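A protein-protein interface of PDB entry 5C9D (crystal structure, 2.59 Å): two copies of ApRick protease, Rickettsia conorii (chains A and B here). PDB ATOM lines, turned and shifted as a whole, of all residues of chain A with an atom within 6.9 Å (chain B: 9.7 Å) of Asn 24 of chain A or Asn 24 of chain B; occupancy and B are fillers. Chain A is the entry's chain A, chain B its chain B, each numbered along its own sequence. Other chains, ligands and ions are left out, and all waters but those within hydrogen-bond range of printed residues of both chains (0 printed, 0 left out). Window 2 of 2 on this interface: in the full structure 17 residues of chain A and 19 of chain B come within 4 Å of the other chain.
OD1 of Asn 24 of chain B sits close to OD1 of Asn 24 of chain A (2.5 Å). OE1 of Glu 83 of chain B lies within salt-bridge range of NZ of Lys 26 of chain A (3.6 Å).
O of Phe 21 of chain A is in hydrogen-bond range of N of Val 79 of chain A (2.8 Å). OG of Ser 77 of chain A sits at hydrogen-bond distance from OE2 of Glu 83 of chain A (2.6 Å). N of Phe 21 of chain B is in hydrogen-bond range of O of Val 79 of chain B. The side-chain hydroxyl (OG) of Ser 77 of chain B sits at hydrogen-bond distance from the side-chain carboxylate (OE2) of Glu 83 of chain B, at 2.8 Å.
Among the printed residues, merely in contact across the chains: Phe 21 of chain A with Asn 24 of chain B, Val 79 of chain A with Phe 21 of chain B, Glu 83 of chain A with Phe 21 of chain B, Phe 21 of chain A with Glu 83 of chain B and Val 79 of chain A with Asn 24 of chain B.
Asn 24 of chain A touches just one residue of chain B: Asn 24 (2.5 Å). Asn 24 of chain B touches just these residues of chain A: Phe 21 (3.6 Å), Asn 24 (2.5 Å) and Val 79 (3.97 Å). No residue of chain B comes within 4 Å of Val 25 of chain A. Of the printed residues of chain A, Phe 21 of chain B touches Val 79 and Glu 83. Printed residues of chain B within 4 Å of Glu 83 of chain A: Phe 21 (3.8 Å). Of the printed residues of chain A, Glu 83 of chain B touches Phe 21 (3.9 Å) and Lys 26 (3.6 Å). Printed residues of chain B within 4 Å of Val 79 of chain A: Phe 21 (3.7 Å) and Asn 24 (3.97 Å). Asn 23 of chain B touches none of the printed residues of chain A. Gly 81 of chain B touches none of the printed residues of chain A. The nearest printed residue of chain B that does not touch Val 79 of chain A is Val 79 of chain B (4.1 Å).
Of the 12 printed residues of chain A, 5 touch a printed residue of chain B. Hydrophobic or aromatic side chains of chain A within 4 Å of the printed part of chain B: Phe 21 and Val 79. Of the 21 printed residues of chain B, 3 touch a printed residue of chain A. Among the printed residues, 7 pairs touch across the chains. Among the printed residues, Asp or Glu carboxylates within 4 Å of a Lys or Arg side-chain nitrogen of the other chain: Lys 26 of chain A with Glu 83 of chain B (3.6 Å).
Phe 21 of chain A touches Asn 24 of chain B, but with the chains exchanged Asn 24 of chain A does not touch Phe 21 of chain B (7.0 Å). Phe 21 of chain A touches Glu 83 of chain B, and with the chains exchanged Glu 83 of chain A touches Phe 21 of chain B. Asn 24 of chain A touches its own counterpart, Asn 24 of chain B. Val 79 of chain A touches Phe 21 of chain B, but with the chains exchanged Phe 21 of chain A does not touch Val 79 of chain B (4.2 Å). Positions printed for both chains: 20, 21, 22, 23, 24, 25, 26, 48, 77, 78, 79 and 83.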
ATOM      1  N   ALA A  20       1.583 -32.525   6.316  1.00  0.00           N
ATOM      2  CA  ALA A  20       2.726 -31.809   5.755  1.00  0.00           C
ATOM      3  C   ALA A  20       3.477 -32.718   4.799  1.00  0.00           C
ATOM      4  O   ALA A  20       3.406 -33.943   4.917  1.00  0.00           O
ATOM      5  CB  ALA A  20       3.633 -31.350   6.881  1.00  0.00           C
ATOM      6  N   PHE A  21       4.179 -32.137   3.831  1.00  0.00           N
ATOM      7  CA  PHE A  21       4.961 -32.937   2.882  1.00  0.00           C
ATOM      8  C   PHE A  21       6.400 -32.821   3.268  1.00  0.00           C
ATOM      9  O   PHE A  21       7.103 -31.876   2.855  1.00  0.00           O
ATOM     10  CB  PHE A  21       4.735 -32.476   1.461  1.00  0.00           C
ATOM     11  CG  PHE A  21       3.331 -32.644   1.031  1.00  0.00           C
ATOM     12  CD1 PHE A  21       2.358 -31.754   1.463  1.00  0.00           C
ATOM     13  CD2 PHE A  21       2.961 -33.709   0.229  1.00  0.00           C
ATOM     14  CE1 PHE A  21       1.038 -31.913   1.084  1.00  0.00           C
ATOM     15  CE2 PHE A  21       1.643 -33.872  -0.166  1.00  0.00           C
ATOM     16  CZ  PHE A  21       0.680 -32.978   0.267  1.00  0.00           C
ATOM     17  N   VAL A  22       6.784 -33.758   4.142  1.00  0.00           N
ATOM     18  CA  VAL A  22       8.168 -33.943   4.562  1.00  0.00           C
ATOM     19  C   VAL A  22       8.802 -34.761   3.485  1.00  0.00           C
ATOM     20  O   VAL A  22       8.349 -35.891   3.211  1.00  0.00           O
ATOM     21  CB  VAL A  22       8.328 -34.715   5.886  1.00  0.00           C
ATOM     22  CG1 VAL A  22       9.815 -34.767   6.300  1.00  0.00           C
ATOM     23  CG2 VAL A  22       7.486 -34.055   6.975  1.00  0.00           C
ATOM     24  N   ASN A  23       9.813 -34.169   2.852  1.00  0.00           N
ATOM     25  CA  ASN A  23      10.579 -34.836   1.802  1.00  0.00           C
ATOM     26  C   ASN A  23       9.617 -35.539   0.838  1.00  0.00           C
ATOM     27  O   ASN A  23       9.811 -36.693   0.468  1.00  0.00           O
ATOM     28  CB  ASN A  23      11.622 -35.773   2.437  1.00  0.00           C
ATOM     29  CG  ASN A  23      12.551 -35.040   3.416  1.00  0.00           C
ATOM     30  OD1 ASN A  23      12.778 -33.839   3.289  1.00  0.00           O
ATOM     31  ND2 ASN A  23      13.082 -35.758   4.394  1.00  0.00           N
ATOM     32  N   ASN A  24       8.553 -34.807   0.491  1.00  0.00           N
ATOM     33  CA  ASN A  24       7.504 -35.234  -0.462  1.00  0.00           C
ATOM     34  C   ASN A  24       6.516 -36.325  -0.008  1.00  0.00           C
ATOM     35  O   ASN A  24       5.606 -36.667  -0.759  1.00  0.00           O
ATOM     36  CB  ASN A  24       8.125 -35.588  -1.811  1.00  0.00           C
ATOM     37  CG  ASN A  24       9.083 -34.515  -2.301  1.00  0.00           C
ATOM     38  OD1 ASN A  24       8.880 -33.326  -2.059  1.00  0.00           O
ATOM     39  ND2 ASN A  24      10.140 -34.934  -2.988  1.00  0.00           N
ATOM     40  N   VAL A  25       6.671 -36.844   1.211  1.00  0.00           N
ATOM     41  CA  VAL A  25       5.707 -37.788   1.791  1.00  0.00           C
ATOM     42  C   VAL A  25       4.812 -37.082   2.796  1.00  0.00           C
ATOM     43  O   VAL A  25       5.281 -36.244   3.583  1.00  0.00           O
ATOM     44  CB  VAL A  25       6.424 -38.894   2.543  1.00  0.00           C
ATOM     45  CG1 VAL A  25       5.424 -39.796   3.245  1.00  0.00           C
ATOM     46  CG2 VAL A  25       7.299 -39.687   1.586  1.00  0.00           C
ATOM     47  N   LYS A  26       3.531 -37.447   2.781  1.00  0.00           N
ATOM     48  CA  LYS A  26       2.483 -36.800   3.614  1.00  0.00           C
ATOM     49  C   LYS A  26       2.377 -37.456   4.997  1.00  0.00           C
ATOM     50  O   LYS A  26       1.865 -38.574   5.131  1.00  0.00           O
ATOM     51  CB  LYS A  26       1.130 -36.889   2.903  1.00  0.00           C
ATOM     52  CG  LYS A  26       0.019 -35.950   3.374  1.00  0.00           C
ATOM     53  CD  LYS A  26      -1.158 -36.121   2.409  1.00  0.00           C
ATOM     54  CE  LYS A  26      -2.276 -35.088   2.542  1.00  0.00           C
ATOM     55  NZ  LYS A  26      -3.445 -35.441   1.649  1.00  0.00           N
ATOM     56  N   LEU A  48       9.806 -42.266   5.719  1.00  0.00           N
ATOM     57  CA  LEU A  48      10.819 -41.350   5.154  1.00  0.00           C
ATOM     58  C   LEU A  48      12.204 -41.995   4.880  1.00  0.00           C
ATOM     59  O   LEU A  48      13.151 -41.315   4.503  1.00  0.00           O
ATOM     60  CB  LEU A  48      10.994 -40.151   6.095  1.00  0.00           C
ATOM     61  CG  LEU A  48       9.728 -39.396   6.524  1.00  0.00           C
ATOM     62  CD1 LEU A  48      10.034 -38.491   7.707  1.00  0.00           C
ATOM     63  CD2 LEU A  48       9.200 -38.571   5.366  1.00  0.00           C
ATOM     64  N   SER A  77      13.215 -31.139   4.103  1.00  0.00           N
ATOM     65  CA  SER A  77      12.195 -30.289   3.516  1.00  0.00           C
ATOM     66  C   SER A  77      10.886 -30.617   4.150  1.00  0.00           C
ATOM     67  O   SER A  77      10.526 -31.778   4.213  1.00  0.00           O
ATOM     68  CB  SER A  77      12.114 -30.586   2.010  1.00  0.00           C
ATOM     69  OG  SER A  77      10.787 -30.480   1.500  1.00  0.00           O
ATOM     70  N   VAL A  78      10.156 -29.609   4.601  1.00  0.00           N
ATOM     71  CA  VAL A  78       8.818 -29.819   5.139  1.00  0.00           C
ATOM     72  C   VAL A  78       7.919 -28.759   4.519  1.00  0.00           C
ATOM     73  O   VAL A  78       8.141 -27.568   4.761  1.00  0.00           O
ATOM     74  CB  VAL A  78       8.750 -29.609   6.667  1.00  0.00           C
ATOM     75  CG1 VAL A  78       7.301 -29.699   7.122  1.00  0.00           C
ATOM     76  CG2 VAL A  78       9.603 -30.622   7.431  1.00  0.00           C
ATOM     77  N   VAL A  79       6.911 -29.177   3.740  1.00  0.00           N
ATOM     78  CA  VAL A  79       6.020 -28.217   3.088  1.00  0.00           C
ATOM     79  C   VAL A  79       4.684 -28.194   3.815  1.00  0.00           C
ATOM     80  O   VAL A  79       4.076 -29.243   4.053  1.00  0.00           O
ATOM     81  CB  VAL A  79       5.829 -28.545   1.602  1.00  0.00           C
ATOM     82  CG1 VAL A  79       4.685 -27.730   0.992  1.00  0.00           C
ATOM     83  CG2 VAL A  79       7.135 -28.303   0.852  1.00  0.00           C
ATOM     84  N   GLU A  83       7.799 -24.072   1.975  1.00  0.00           N
ATOM     85  CA  GLU A  83       8.756 -25.123   2.260  1.00  0.00           C
ATOM     86  C   GLU A  83       9.618 -24.655   3.431  1.00  0.00           C
ATOM     87  O   GLU A  83      10.250 -23.592   3.360  1.00  0.00           O
ATOM     88  CB  GLU A  83       9.644 -25.421   1.067  1.00  0.00           C
ATOM     89  CG  GLU A  83      10.600 -26.555   1.355  1.00  0.00           C
ATOM     90  CD  GLU A  83      11.205 -27.144   0.113  1.00  0.00           C
ATOM     91  OE1 GLU A  83      11.583 -26.372  -0.784  1.00  0.00           O
ATOM     92  OE2 GLU A  83      11.304 -28.385   0.028  1.00  0.00           O
ATOM     93  N   ASN B  19       5.054 -19.413  -5.587  1.00  0.00           N
ATOM     94  CA  ASN B  19       5.577 -20.751  -5.715  1.00  0.00           C
ATOM     95  C   ASN B  19       4.522 -21.705  -5.199  1.00  0.00           C
ATOM     96  O   ASN B  19       3.961 -21.512  -4.109  1.00  0.00           O
ATOM     97  CB  ASN B  19       6.860 -20.895  -4.933  1.00  0.00           C
ATOM     98  CG  ASN B  19       7.950 -19.964  -5.423  1.00  0.00           C
ATOM     99  OD1 ASN B  19       8.555 -20.230  -6.456  1.00  0.00           O
ATOM    100  ND2 ASN B  19       8.234 -18.883  -4.668  1.00  0.00           N
ATOM    101  N   ALA B  20       4.209 -22.690  -6.029  1.00  0.00           N
ATOM    102  CA  ALA B  20       3.320 -23.751  -5.661  1.00  0.00           C
ATOM    103  C   ALA B  20       4.109 -25.031  -5.805  1.00  0.00           C
ATOM    104  O   ALA B  20       5.131 -25.078  -6.485  1.00  0.00           O
ATOM    105  CB  ALA B  20       2.110 -23.768  -6.558  1.00  0.00           C
ATOM    106  N   PHE B  21       3.604 -26.060  -5.145  1.00  0.00           N
ATOM    107  CA  PHE B  21       4.192 -27.371  -5.103  1.00  0.00           C
ATOM    108  C   PHE B  21       3.212 -28.247  -5.843  1.00  0.00           C
ATOM    109  O   PHE B  21       2.315 -28.867  -5.282  1.00  0.00           O
ATOM    110  CB  PHE B  21       4.388 -27.755  -3.626  1.00  0.00           C
ATOM    111  CG  PHE B  21       5.234 -26.765  -2.885  1.00  0.00           C
ATOM    112  CD1 PHE B  21       6.619 -26.806  -2.996  1.00  0.00           C
ATOM    113  CD2 PHE B  21       4.658 -25.730  -2.175  1.00  0.00           C
ATOM    114  CE1 PHE B  21       7.411 -25.850  -2.374  1.00  0.00           C
ATOM    115  CE2 PHE B  21       5.440 -24.780  -1.542  1.00  0.00           C
ATOM    116  CZ  PHE B  21       6.821 -24.835  -1.652  1.00  0.00           C
ATOM    117  N   VAL B  22       3.349 -28.220  -7.150  1.00  0.00           N
ATOM    118  CA  VAL B  22       2.561 -29.060  -8.024  1.00  0.00           C
ATOM    119  C   VAL B  22       3.079 -30.480  -7.959  1.00  0.00           C
ATOM    120  O   VAL B  22       4.205 -30.753  -8.408  1.00  0.00           O
ATOM    121  CB  VAL B  22       2.644 -28.573  -9.447  1.00  0.00           C
ATOM    122  CG1 VAL B  22       1.789 -29.454 -10.341  1.00  0.00           C
ATOM    123  CG2 VAL B  22       2.154 -27.134  -9.493  1.00  0.00           C
ATOM    124  N   ASN B  23       2.276 -31.379  -7.382  1.00  0.00           N
ATOM    125  CA  ASN B  23       2.728 -32.746  -7.114  1.00  0.00           C
ATOM    126  C   ASN B  23       4.071 -32.709  -6.406  1.00  0.00           C
ATOM    127  O   ASN B  23       5.027 -33.346  -6.831  1.00  0.00           O
ATOM    128  CB  ASN B  23       2.823 -33.523  -8.413  1.00  0.00           C
ATOM    129  CG  ASN B  23       1.516 -33.522  -9.173  1.00  0.00           C
ATOM    130  OD1 ASN B  23       0.449 -33.394  -8.579  1.00  0.00           O
ATOM    131  ND2 ASN B  23       1.592 -33.660 -10.489  1.00  0.00           N
ATOM    132  N   ASN B  24       4.090 -31.958  -5.301  1.00  0.00           N
ATOM    133  CA  ASN B  24       5.292 -31.543  -4.560  1.00  0.00           C
ATOM    134  C   ASN B  24       6.590 -31.324  -5.319  1.00  0.00           C
ATOM    135  O   ASN B  24       7.658 -31.780  -4.906  1.00  0.00           O
ATOM    136  CB  ASN B  24       5.526 -32.381  -3.302  1.00  0.00           C
ATOM    137  CG  ASN B  24       5.956 -31.516  -2.127  1.00  0.00           C
ATOM    138  OD1 ASN B  24       7.116 -31.529  -1.701  1.00  0.00           O
ATOM    139  ND2 ASN B  24       5.018 -30.711  -1.627  1.00  0.00           N
ATOM    140  N   VAL B  25       6.461 -30.615  -6.438  1.00  0.00           N
ATOM    141  CA  VAL B  25       7.583 -30.031  -7.138  1.00  0.00           C
ATOM    142  C   VAL B  25       7.341 -28.539  -7.109  1.00  0.00           C
ATOM    143  O   VAL B  25       6.296 -28.076  -7.569  1.00  0.00           O
ATOM    144  CB  VAL B  25       7.673 -30.544  -8.581  1.00  0.00           C
ATOM    145  CG1 VAL B  25       8.297 -29.518  -9.523  1.00  0.00           C
ATOM    146  CG2 VAL B  25       8.465 -31.832  -8.605  1.00  0.00           C
ATOM    147  N   LYS B  26       8.289 -27.797  -6.532  1.00  0.00           N
ATOM    148  CA  LYS B  26       8.187 -26.349  -6.452  1.00  0.00           C
ATOM    149  C   LYS B  26       8.280 -25.775  -7.869  1.00  0.00           C
ATOM    150  O   LYS B  26       9.341 -25.760  -8.491  1.00  0.00           O
ATOM    151  CB  LYS B  26       9.274 -25.762  -5.546  1.00  0.00           C
ATOM    152  CG  LYS B  26       9.032 -24.308  -5.175  1.00  0.00           C
ATOM    153  CD  LYS B  26      10.033 -23.820  -4.140  1.00  0.00           C
ATOM    154  CE  LYS B  26       9.489 -22.623  -3.363  1.00  0.00           C
ATOM    155  NZ  LYS B  26      10.174 -22.383  -2.055  1.00  0.00           N
ATOM    156  N   ILE B  27       7.141 -25.355  -8.394  1.00  0.00           N
ATOM    157  CA  ILE B  27       7.106 -24.648  -9.643  1.00  0.00           C
ATOM    158  C   ILE B  27       6.856 -23.183  -9.292  1.00  0.00           C
ATOM    159  O   ILE B  27       6.148 -22.872  -8.309  1.00  0.00           O
ATOM    160  CB  ILE B  27       6.005 -25.210 -10.556  1.00  0.00           C
ATOM    161  CG1 ILE B  27       6.342 -26.651 -10.945  1.00  0.00           C
ATOM    162  CG2 ILE B  27       5.803 -24.326 -11.780  1.00  0.00           C
ATOM    163  CD1 ILE B  27       7.775 -26.819 -11.376  1.00  0.00           C
ATOM    164  N   LYS B  47      10.102 -31.180 -15.995  1.00  0.00           N
ATOM    165  CA  LYS B  47      10.455 -31.162 -14.557  1.00  0.00           C
ATOM    166  C   LYS B  47       9.443 -31.925 -13.678  1.00  0.00           C
ATOM    167  O   LYS B  47       9.799 -32.487 -12.646  1.00  0.00           O
ATOM    168  CB  LYS B  47      10.549 -29.704 -14.108  1.00  0.00           C
ATOM    169  CG  LYS B  47      10.779 -29.414 -12.638  1.00  0.00           C
ATOM    170  CD  LYS B  47      10.840 -27.898 -12.488  1.00  0.00           C
ATOM    171  CE  LYS B  47      11.005 -27.429 -11.052  1.00  0.00           C
ATOM    172  NZ  LYS B  47      10.823 -25.949 -10.920  1.00  0.00           N
ATOM    173  N   LEU B  48       8.182 -31.941 -14.096  1.00  0.00           N
ATOM    174  CA  LEU B  48       7.144 -32.675 -13.390  1.00  0.00           C
ATOM    175  C   LEU B  48       7.024 -34.082 -13.964  1.00  0.00           C
ATOM    176  O   LEU B  48       6.000 -34.743 -13.785  1.00  0.00           O
ATOM    177  CB  LEU B  48       5.802 -31.941 -13.529  1.00  0.00           C
ATOM    178  CG  LEU B  48       5.732 -30.548 -12.890  1.00  0.00           C
ATOM    179  CD1 LEU B  48       4.808 -29.615 -13.652  1.00  0.00           C
ATOM    180  CD2 LEU B  48       5.314 -30.625 -11.429  1.00  0.00           C
ATOM    181  N   LEU B  75      -3.572 -31.501 -12.810  1.00  0.00           N
ATOM    182  CA  LEU B  75      -2.611 -31.514 -11.762  1.00  0.00           C
ATOM    183  C   LEU B  75      -3.225 -32.191 -10.549  1.00  0.00           C
ATOM    184  O   LEU B  75      -4.281 -31.785 -10.092  1.00  0.00           O
ATOM    185  CB  LEU B  75      -2.188 -30.101 -11.450  1.00  0.00           C
ATOM    186  CG  LEU B  75      -1.514 -29.457 -12.669  1.00  0.00           C
ATOM    187  CD1 LEU B  75      -1.137 -28.005 -12.384  1.00  0.00           C
ATOM    188  CD2 LEU B  75      -0.299 -30.267 -13.095  1.00  0.00           C
ATOM    189  N   ASN B  76      -2.559 -33.228 -10.038  1.00  0.00           N
ATOM    190  CA  ASN B  76      -3.082 -33.993  -8.904  1.00  0.00           C
ATOM    191  C   ASN B  76      -3.088 -33.251  -7.571  1.00  0.00           C
ATOM    192  O   ASN B  76      -4.046 -33.347  -6.807  1.00  0.00           O
ATOM    193  CB  ASN B  76      -2.297 -35.284  -8.725  1.00  0.00           C
ATOM    194  CG  ASN B  76      -3.169 -36.419  -8.255  1.00  0.00           C
ATOM    195  OD1 ASN B  76      -4.376 -36.260  -8.082  1.00  0.00           O
ATOM    196  ND2 ASN B  76      -2.566 -37.582  -8.062  1.00  0.00           N
ATOM    197  N   SER B  77      -2.004 -32.534  -7.300  1.00  0.00           N
ATOM    198  CA  SER B  77      -1.816 -31.781  -6.065  1.00  0.00           C
ATOM    199  C   SER B  77      -1.218 -30.430  -6.393  1.00  0.00           C
ATOM    200  O   SER B  77      -0.201 -30.337  -7.074  1.00  0.00           O
ATOM    201  CB  SER B  77      -0.831 -32.515  -5.140  1.00  0.00           C
ATOM    202  OG  SER B  77      -0.371 -31.676  -4.073  1.00  0.00           O
ATOM    203  N   VAL B  78      -1.816 -29.375  -5.890  1.00  0.00           N
ATOM    204  CA  VAL B  78      -1.197 -28.074  -6.039  1.00  0.00           C
ATOM    205  C   VAL B  78      -1.274 -27.385  -4.692  1.00  0.00           C
ATOM    206  O   VAL B  78      -2.339 -26.946  -4.299  1.00  0.00           O
ATOM    207  CB  VAL B  78      -1.857 -27.281  -7.160  1.00  0.00           C
ATOM    208  CG1 VAL B  78      -1.289 -25.871  -7.243  1.00  0.00           C
ATOM    209  CG2 VAL B  78      -1.643 -28.015  -8.478  1.00  0.00           C
ATOM    210  N   VAL B  79      -0.133 -27.348  -3.989  1.00  0.00           N
ATOM    211  CA  VAL B  79      -0.027 -26.789  -2.642  1.00  0.00           C
ATOM    212  C   VAL B  79       0.518 -25.366  -2.720  1.00  0.00           C
ATOM    213  O   VAL B  79       1.634 -25.151  -3.192  1.00  0.00           O
ATOM    214  CB  VAL B  79       0.968 -27.590  -1.767  1.00  0.00           C
ATOM    215  CG1 VAL B  79       0.844 -27.199  -0.284  1.00  0.00           C
ATOM    216  CG2 VAL B  79       0.785 -29.084  -1.970  1.00  0.00           C
ATOM    217  N   ILE B  80      -0.268 -24.388  -2.299  1.00  0.00           N
ATOM    218  CA  ILE B  80       0.310 -23.092  -1.923  1.00  0.00           C
ATOM    219  C   ILE B  80       0.414 -23.131  -0.395  1.00  0.00           C
ATOM    220  O   ILE B  80       1.327 -22.552   0.202  1.00  0.00           O
ATOM    221  CB  ILE B  80      -0.515 -21.847  -2.323  1.00  0.00           C
ATOM    222  CG1 ILE B  80      -1.355 -22.029  -3.606  1.00  0.00           C
ATOM    223  CG2 ILE B  80       0.436 -20.660  -2.425  1.00  0.00           C
ATOM    224  CD1 ILE B  80      -0.602 -21.928  -4.919  1.00  0.00           C
ATOM    225  N   GLY B  81      -0.584 -23.779   0.212  1.00  0.00           N
ATOM    226  CA  GLY B  81      -0.521 -24.303   1.583  1.00  0.00           C
ATOM    227  C   GLY B  81      -1.627 -25.312   1.850  1.00  0.00           C
ATOM    228  O   GLY B  81      -1.396 -26.394   2.439  1.00  0.00           O
ATOM    229  N   LYS B  82      -2.837 -24.908   1.446  1.00  0.00           N
ATOM    230  CA  LYS B  82      -3.919 -25.828   1.189  1.00  0.00           C
ATOM    231  C   LYS B  82      -3.370 -26.623   0.039  1.00  0.00           C
ATOM    232  O   LYS B  82      -2.538 -26.121  -0.724  1.00  0.00           O
ATOM    233  CB  LYS B  82      -5.251 -25.110   0.807  1.00  0.00           C
ATOM    234  CG  LYS B  82      -6.348 -26.010   0.195  1.00  0.00           C
ATOM    235  CD  LYS B  82      -7.733 -25.884   0.838  1.00  0.00           C
ATOM    236  CE  LYS B  82      -8.442 -24.605   0.406  1.00  0.00           C
ATOM    237  NZ  LYS B  82      -9.684 -24.269   1.170  1.00  0.00           N
ATOM    238  N   GLU B  83      -3.793 -27.877  -0.038  1.00  0.00           N
ATOM    239  CA  GLU B  83      -3.591 -28.677  -1.221  1.00  0.00           C
ATOM    240  C   GLU B  83      -4.906 -28.738  -2.014  1.00  0.00           C
ATOM    241  O   GLU B  83      -5.944 -29.200  -1.518  1.00  0.00           O
ATOM    242  CB  GLU B  83      -3.116 -30.080  -0.853  1.00  0.00           C
ATOM    243  CG  GLU B  83      -2.631 -30.871  -2.059  1.00  0.00           C
ATOM    244  CD  GLU B  83      -2.743 -32.367  -1.880  1.00  0.00           C
ATOM    245  OE1 GLU B  83      -3.121 -32.828  -0.776  1.00  0.00           O
ATOM    246  OE2 GLU B  83      -2.446 -33.077  -2.861  1.00  0.00           O
ATOM    247  N   PHE B  84      -4.843 -28.236  -3.238  1.00  0.00           N
ATOM    248  CA  PHE B  84      -5.933 -28.340  -4.175  1.00  0.00           C
ATOM    249  C   PHE B  84      -5.690 -29.548  -5.063  1.00  0.00           C
ATOM    250  O   PHE B  84      -4.603 -29.711  -5.637  1.00  0.00           O
ATOM    251  CB  PHE B  84      -6.010 -27.073  -5.008  1.00  0.00           C
ATOM    252  CG  PHE B  84      -6.388 -25.856  -4.206  1.00  0.00           C
ATOM    253  CD1 PHE B  84      -7.711 -25.635  -3.843  1.00  0.00           C
ATOM    254  CD2 PHE B  84      -5.425 -24.938  -3.802  1.00  0.00           C
ATOM    255  CE1 PHE B  84      -8.062 -24.518  -3.103  1.00  0.00           C
ATOM    256  CE2 PHE B  84      -5.777 -23.820  -3.065  1.00  0.00           C
ATOM    257  CZ  PHE B  84      -7.089 -23.614  -2.706  1.00  0.00           C
